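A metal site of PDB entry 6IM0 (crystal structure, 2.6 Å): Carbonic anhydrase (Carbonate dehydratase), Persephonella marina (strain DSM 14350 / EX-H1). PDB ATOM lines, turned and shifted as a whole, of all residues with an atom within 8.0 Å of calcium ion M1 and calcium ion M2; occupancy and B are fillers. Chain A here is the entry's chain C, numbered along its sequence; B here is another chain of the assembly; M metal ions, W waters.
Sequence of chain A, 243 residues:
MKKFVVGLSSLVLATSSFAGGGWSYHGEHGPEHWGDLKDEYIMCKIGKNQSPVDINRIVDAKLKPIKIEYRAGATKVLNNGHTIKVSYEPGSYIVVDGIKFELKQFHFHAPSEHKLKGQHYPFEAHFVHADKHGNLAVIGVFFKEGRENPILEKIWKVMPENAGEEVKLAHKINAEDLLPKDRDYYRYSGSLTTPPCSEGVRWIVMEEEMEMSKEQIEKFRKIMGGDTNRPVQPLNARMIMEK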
ATOM      1  N   TYR A 121      21.993  33.110  13.756  1.00  0.00           N
ATOM      2  CA  TYR A 121      23.375  32.650  13.548  1.00  0.00           C
ATOM      3  C   TYR A 121      24.233  33.912  13.514  1.00  0.00           C
ATOM      4  O   TYR A 121      23.714  35.005  13.263  1.00  0.00           O
ATOM      5  CB  TYR A 121      23.502  31.895  12.244  1.00  0.00           C
ATOM      6  CG  TYR A 121      22.919  30.492  12.244  1.00  0.00           C
ATOM      7  CD1 TYR A 121      21.553  30.300  11.988  1.00  0.00           C
ATOM      8  CD2 TYR A 121      23.715  29.374  12.428  1.00  0.00           C
ATOM      9  CE1 TYR A 121      21.019  29.014  11.919  1.00  0.00           C
ATOM     10  CE2 TYR A 121      23.177  28.105  12.396  1.00  0.00           C
ATOM     11  CZ  TYR A 121      21.839  27.930  12.139  1.00  0.00           C
ATOM     12  OH  TYR A 121      21.280  26.667  12.108  1.00  0.00           O
ATOM     13  N   PHE A 142      23.410  29.979   6.269  1.00  0.00           N
ATOM     14  CA  PHE A 142      23.828  30.343   7.614  1.00  0.00           C
ATOM     15  C   PHE A 142      25.263  29.875   7.848  1.00  0.00           C
ATOM     16  O   PHE A 142      25.657  28.819   7.403  1.00  0.00           O
ATOM     17  CB  PHE A 142      22.944  29.669   8.676  1.00  0.00           C
ATOM     18  CG  PHE A 142      21.533  30.131   8.689  1.00  0.00           C
ATOM     19  CD1 PHE A 142      21.218  31.466   8.914  1.00  0.00           C
ATOM     20  CD2 PHE A 142      20.475  29.216   8.510  1.00  0.00           C
ATOM     21  CE1 PHE A 142      19.883  31.885   8.951  1.00  0.00           C
ATOM     22  CE2 PHE A 142      19.161  29.615   8.541  1.00  0.00           C
ATOM     23  CZ  PHE A 142      18.854  30.957   8.769  1.00  0.00           C
ATOM     24  N   LYS A 144      27.953  29.290  11.220  1.00  0.00           N
ATOM     25  CA  LYS A 144      28.276  29.325  12.670  1.00  0.00           C
ATOM     26  C   LYS A 144      29.801  29.471  12.904  1.00  0.00           C
ATOM     27  O   LYS A 144      30.583  29.303  11.970  1.00  0.00           O
ATOM     28  CB  LYS A 144      27.768  28.058  13.360  1.00  0.00           C
ATOM     29  CG  LYS A 144      28.413  26.753  12.903  1.00  0.00           C
ATOM     30  CD  LYS A 144      28.134  25.630  13.905  1.00  0.00           C
ATOM     31  CE  LYS A 144      28.656  24.292  13.402  1.00  0.00           C
ATOM     32  NZ  LYS A 144      28.402  23.176  14.367  1.00  0.00           N
ATOM     33  N   PRO A 180      26.414  24.008   1.390  1.00  0.00           N
ATOM     34  CA  PRO A 180      26.500  22.698   1.977  1.00  0.00           C
ATOM     35  C   PRO A 180      26.277  21.585   0.975  1.00  0.00           C
ATOM     36  O   PRO A 180      25.780  21.841  -0.117  1.00  0.00           O
ATOM     37  CB  PRO A 180      25.400  22.723   3.039  1.00  0.00           C
ATOM     38  CG  PRO A 180      24.433  23.736   2.583  1.00  0.00           C
ATOM     39  CD  PRO A 180      25.255  24.776   1.896  1.00  0.00           C
ATOM     40  N   LYS A 181      26.670  20.380   1.353  1.00  0.00           N
ATOM     41  CA  LYS A 181      26.446  19.167   0.561  1.00  0.00           C
ATOM     42  C   LYS A 181      25.059  18.586   0.792  1.00  0.00           C
ATOM     43  O   LYS A 181      24.477  18.100  -0.134  1.00  0.00           O
ATOM     44  CB  LYS A 181      27.529  18.113   0.852  1.00  0.00           C
ATOM     45  CG  LYS A 181      28.735  18.244  -0.066  1.00  0.00           C
ATOM     46  CD  LYS A 181      30.086  17.978   0.619  1.00  0.00           C
ATOM     47  CE  LYS A 181      31.226  17.803  -0.399  1.00  0.00           C
ATOM     48  NZ  LYS A 181      31.329  18.905  -1.427  1.00  0.00           N
ATOM     49  N   ASP A 182      24.545  18.673   2.023  1.00  0.00           N
ATOM     50  CA  ASP A 182      23.092  18.488   2.318  1.00  0.00           C
ATOM     51  C   ASP A 182      22.403  19.737   1.722  1.00  0.00           C
ATOM     52  O   ASP A 182      22.634  20.863   2.172  1.00  0.00           O
ATOM     53  CB  ASP A 182      22.794  18.355   3.865  1.00  0.00           C
ATOM     54  CG  ASP A 182      21.347  17.789   4.192  1.00  0.00           C
ATOM     55  OD1 ASP A 182      20.594  17.419   3.259  1.00  0.00           O
ATOM     56  OD2 ASP A 182      20.951  17.697   5.391  1.00  0.00           O
ATOM     57  N   GLU A 207      19.088  24.477   5.021  1.00  0.00           N
ATOM     58  CA  GLU A 207      18.922  24.001   6.413  1.00  0.00           C
ATOM     59  C   GLU A 207      20.239  23.791   7.083  1.00  0.00           C
ATOM     60  O   GLU A 207      20.383  24.045   8.263  1.00  0.00           O
ATOM     61  CB  GLU A 207      18.116  22.708   6.495  1.00  0.00           C
ATOM     62  CG  GLU A 207      16.693  22.813   5.957  1.00  0.00           C
ATOM     63  CD  GLU A 207      15.917  21.497   6.023  1.00  0.00           C
ATOM     64  OE1 GLU A 207      15.132  21.220   5.057  1.00  0.00           O
ATOM     65  OE2 GLU A 207      16.078  20.753   7.029  1.00  0.00           O
ATOM     66  N   GLU A 208      21.216  23.292   6.337  1.00  0.00           N
ATOM     67  CA  GLU A 208      22.508  23.003   6.910  1.00  0.00           C
ATOM     68  C   GLU A 208      23.388  24.245   6.871  1.00  0.00           C
ATOM     69  O   GLU A 208      23.566  24.875   5.826  1.00  0.00           O
ATOM     70  CB  GLU A 208      23.177  21.801   6.215  1.00  0.00           C
ATOM     71  CG  GLU A 208      24.575  21.420   6.724  1.00  0.00           C
ATOM     72  CD  GLU A 208      24.641  21.104   8.199  1.00  0.00           C
ATOM     73  OE1 GLU A 208      23.633  20.677   8.815  1.00  0.00           O
ATOM     74  OE2 GLU A 208      25.733  21.260   8.766  1.00  0.00           O
ATOM     75  N   GLU A 209      23.923  24.572   8.043  1.00  0.00           N
ATOM     76  CA  GLU A 209      24.825  25.695   8.209  1.00  0.00           C
ATOM     77  C   GLU A 209      26.241  25.339   7.743  1.00  0.00           C
ATOM     78  O   GLU A 209      26.625  24.161   7.734  1.00  0.00           O
ATOM     79  CB  GLU A 209      24.859  26.129   9.690  1.00  0.00           C
ATOM     80  CG  GLU A 209      25.786  25.327  10.636  1.00  0.00           C
ATOM     81  CD  GLU A 209      25.503  23.834  10.688  1.00  0.00           C
ATOM     82  OE1 GLU A 209      24.310  23.462  10.823  1.00  0.00           O
ATOM     83  OE2 GLU A 209      26.481  23.041  10.625  1.00  0.00           O
ATOM     84  N   MET A 210      27.023  26.373   7.499  1.00  0.00           N
ATOM     85  CA  MET A 210      28.438  26.251   7.173  1.00  0.00           C
ATOM     86  C   MET A 210      29.209  26.859   8.323  1.00  0.00           C
ATOM     87  O   MET A 210      28.596  27.365   9.260  1.00  0.00           O
ATOM     88  CB  MET A 210      28.734  26.984   5.878  1.00  0.00           C
ATOM     89  CG  MET A 210      28.091  26.354   4.658  1.00  0.00           C
ATOM     90  SD  MET A 210      28.596  24.668   4.260  1.00  0.00           S
ATOM     91  CE  MET A 210      30.087  24.981   3.331  1.00  0.00           C
ATOM     92  N   GLU A 211      30.540  26.795   8.245  1.00  0.00           N
ATOM     93  CA  GLU A 211      31.420  27.241   9.315  1.00  0.00           C
ATOM     94  C   GLU A 211      32.335  28.365   8.883  1.00  0.00           C
ATOM     95  O   GLU A 211      32.761  28.460   7.741  1.00  0.00           O
ATOM     96  CB  GLU A 211      32.301  26.114   9.784  1.00  0.00           C
ATOM     97  CG  GLU A 211      31.641  25.080  10.683  1.00  0.00           C
ATOM     98  CD  GLU A 211      32.662  24.119  11.291  1.00  0.00           C
ATOM     99  OE1 GLU A 211      33.549  23.676  10.524  1.00  0.00           O
ATOM    100  OE2 GLU A 211      32.584  23.812  12.519  1.00  0.00           O
ATOM    101  N   ILE B  58      26.684  20.579  18.767  1.00  0.00           N
ATOM    102  CA  ILE B  58      26.436  19.711  17.649  1.00  0.00           C
ATOM    103  C   ILE B  58      27.630  19.788  16.710  1.00  0.00           C
ATOM    104  O   ILE B  58      28.139  20.865  16.421  1.00  0.00           O
ATOM    105  CB  ILE B  58      25.170  20.148  16.897  1.00  0.00           C
ATOM    106  CG1 ILE B  58      23.988  20.201  17.854  1.00  0.00           C
ATOM    107  CG2 ILE B  58      24.883  19.200  15.746  1.00  0.00           C
ATOM    108  CD1 ILE B  58      22.734  20.890  17.303  1.00  0.00           C
ATOM    109  N   VAL B  59      28.026  18.650  16.181  1.00  0.00           N
ATOM    110  CA  VAL B  59      29.048  18.657  15.187  1.00  0.00           C
ATOM    111  C   VAL B  59      28.620  17.798  14.022  1.00  0.00           C
ATOM    112  O   VAL B  59      28.151  16.686  14.206  1.00  0.00           O
ATOM    113  CB  VAL B  59      30.393  18.251  15.798  1.00  0.00           C
ATOM    114  CG1 VAL B  59      30.356  16.845  16.282  1.00  0.00           C
ATOM    115  CG2 VAL B  59      31.536  18.423  14.802  1.00  0.00           C
ATOM    116  N   ASP B  60      28.831  18.292  12.813  1.00  0.00           N
ATOM    117  CA  ASP B  60      28.591  17.511  11.621  1.00  0.00           C
ATOM    118  C   ASP B  60      29.511  16.300  11.645  1.00  0.00           C
ATOM    119  O   ASP B  60      30.693  16.406  11.968  1.00  0.00           O
ATOM    120  CB  ASP B  60      28.827  18.363  10.365  1.00  0.00           C
ATOM    121  CG  ASP B  60      27.919  19.572  10.288  1.00  0.00           C
ATOM    122  OD1 ASP B  60      26.735  19.481  10.667  1.00  0.00           O
ATOM    123  OD2 ASP B  60      28.357  20.621   9.799  1.00  0.00           O
ATOM    124  N   ALA B  61      28.970  15.150  11.304  1.00  0.00           N
ATOM    125  CA  ALA B  61      29.739  13.922  11.209  1.00  0.00           C
ATOM    126  C   ALA B  61      29.212  12.995  10.116  1.00  0.00           C
ATOM    127  O   ALA B  61      28.029  12.957   9.872  1.00  0.00           O
ATOM    128  CB  ALA B  61      29.708  13.217  12.542  1.00  0.00           C
ATOM    129  N   LYS B 117      18.485  22.722  20.825  1.00  0.00           N
ATOM    130  CA  LYS B 117      18.998  24.087  20.964  1.00  0.00           C
ATOM    131  C   LYS B 117      18.166  24.917  21.934  1.00  0.00           C
ATOM    132  O   LYS B 117      17.649  25.975  21.595  1.00  0.00           O
ATOM    133  CB  LYS B 117      19.163  24.743  19.574  1.00  0.00           C
ATOM    134  CG  LYS B 117      20.477  24.335  18.928  1.00  0.00           C
ATOM    135  CD  LYS B 117      20.701  24.892  17.529  1.00  0.00           C
ATOM    136  CE  LYS B 117      22.175  24.921  17.169  1.00  0.00           C
ATOM    137  NZ  LYS B 117      22.382  24.936  15.686  1.00  0.00           N
ATOM    138  N   TYR B 186      20.668  12.627  14.886  1.00  0.00           N
ATOM    139  CA  TYR B 186      21.663  12.962  15.884  1.00  0.00           C
ATOM    140  C   TYR B 186      22.065  11.702  16.639  1.00  0.00           C
ATOM    141  O   TYR B 186      21.218  10.867  16.950  1.00  0.00           O
ATOM    142  CB  TYR B 186      21.138  13.954  16.902  1.00  0.00           C
ATOM    143  CG  TYR B 186      20.662  15.245  16.301  1.00  0.00           C
ATOM    144  CD1 TYR B 186      21.563  16.186  15.810  1.00  0.00           C
ATOM    145  CD2 TYR B 186      19.308  15.558  16.254  1.00  0.00           C
ATOM    146  CE1 TYR B 186      21.138  17.380  15.274  1.00  0.00           C
ATOM    147  CE2 TYR B 186      18.860  16.754  15.728  1.00  0.00           C
ATOM    148  CZ  TYR B 186      19.776  17.655  15.224  1.00  0.00           C
ATOM    149  OH  TYR B 186      19.303  18.829  14.676  1.00  0.00           O
ATOM    150  N   GLU B 207      16.337  13.778  13.221  1.00  0.00           N
ATOM    151  CA  GLU B 207      16.248  15.237  12.990  1.00  0.00           C
ATOM    152  C   GLU B 207      14.864  15.677  12.548  1.00  0.00           C
ATOM    153  O   GLU B 207      14.410  16.720  12.960  1.00  0.00           O
ATOM    154  CB  GLU B 207      17.232  15.718  11.931  1.00  0.00           C
ATOM    155  CG  GLU B 207      18.685  15.426  12.264  1.00  0.00           C
ATOM    156  CD  GLU B 207      19.658  15.870  11.180  1.00  0.00           C
ATOM    157  OE1 GLU B 207      20.660  15.149  10.943  1.00  0.00           O
ATOM    158  OE2 GLU B 207      19.403  16.952  10.578  1.00  0.00           O
ATOM    159  N   MET B 241      26.661  14.286  17.577  1.00  0.00           N
ATOM    160  CA  MET B 241      26.932  14.156  16.166  1.00  0.00           C
ATOM    161  C   MET B 241      25.653  14.312  15.340  1.00  0.00           C
ATOM    162  O   MET B 241      24.617  13.742  15.686  1.00  0.00           O
ATOM    163  CB  MET B 241      27.536  12.806  15.891  1.00  0.00           C
ATOM    164  CG  MET B 241      28.876  12.597  16.542  1.00  0.00           C
ATOM    165  SD  MET B 241      29.110  10.857  16.963  1.00  0.00           S
ATOM    166  CE  MET B 241      30.584  10.719  16.070  1.00  0.00           C
ATOM    167  N   GLU B 242      25.762  15.022  14.211  1.00  0.00           N
ATOM    168  CA  GLU B 242      24.668  15.250  13.249  1.00  0.00           C
ATOM    169  C   GLU B 242      25.017  14.717  11.858  1.00  0.00           C
ATOM    170  O   GLU B 242      26.032  15.117  11.254  1.00  0.00           O
ATOM    171  CB  GLU B 242      24.378  16.736  13.104  1.00  0.00           C
ATOM    172  CG  GLU B 242      23.194  17.037  12.181  1.00  0.00           C
ATOM    173  CD  GLU B 242      23.038  18.494  11.781  1.00  0.00           C
ATOM    174  OE1 GLU B 242      23.574  19.403  12.451  1.00  0.00           O
ATOM    175  OE2 GLU B 242      22.354  18.751  10.766  1.00  0.00           O
ATOM    176  N   LYS B 243      24.167  13.852  11.321  1.00  0.00           N
ATOM    177  CA  LYS B 243      24.359  13.278  10.005  1.00  0.00           C
ATOM    178  C   LYS B 243      24.136  14.280   8.841  1.00  0.00           C
ATOM    179  O   LYS B 243      23.121  14.984   8.792  1.00  0.00           O
ATOM    180  CB  LYS B 243      23.442  12.074   9.851  1.00  0.00           C
ATOM    181  CG  LYS B 243      23.739  11.246   8.624  1.00  0.00           C
ATOM    182  CD  LYS B 243      22.879  10.025   8.544  1.00  0.00           C
ATOM    183  CE  LYS B 243      23.210   9.171   7.332  1.00  0.00           C
ATOM    184  NZ  LYS B 243      22.801   9.826   6.064  1.00  0.00           N
HETATM  185 CA    CA M   1      27.886  22.164   8.403  1.00  0.00          CA
HETATM  186 CA    CA M   2      24.932  21.036  11.106  1.00  0.00          CA
HETATM  187  O   HOH W   1      30.239  23.357   8.488  1.00  0.00           O
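The backbone NH of Glu 242 of chain B is in hydrogen-bond range of the backbone carbonyl oxygen of Val 59 of chain B (2.9 Å).
The backbone carbonyl oxygen of Glu 242 of chain B sits at hydrogen-bond distance from the backbone NH of Ala 61 of chain B, 2.9 Å away.
Within 4 Å of calcium ion M1: Glu 208, Glu 209 and Asp 60 of chain B.
Within 4 Å of calcium ion M2: Glu 208, Glu 209, Asp 60 of chain B and Glu 242 of chain B.
Calcium ion M1 is bound by the side-chain carboxylate (OD2) of Asp 60 of chain B (2.1 Å), the side-chain carboxylate (OE2) of Glu 208 (2.4 Å), the backbone carbonyl oxygen (O) of Glu 209 (2.5 Å), water W1 (2.6 Å) and the side-chain carboxylate (OE2) of Glu 209 (2.8 Å).
Calcium ion M1 has five donor atoms within binding distance.
Calcium ion M2 is bound by the side-chain carboxylate (OD1) of Asp 60 of chain B, the side-chain carboxylate (OE2) of Glu 208, the side-chain carboxylate (OE1) of Glu 242 of chain B, the side-chain carboxylate (OE1) of Glu 209, the side-chain carboxylate (OE2) of Glu 209 and the side-chain carboxylate (OE1) of Glu 208.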
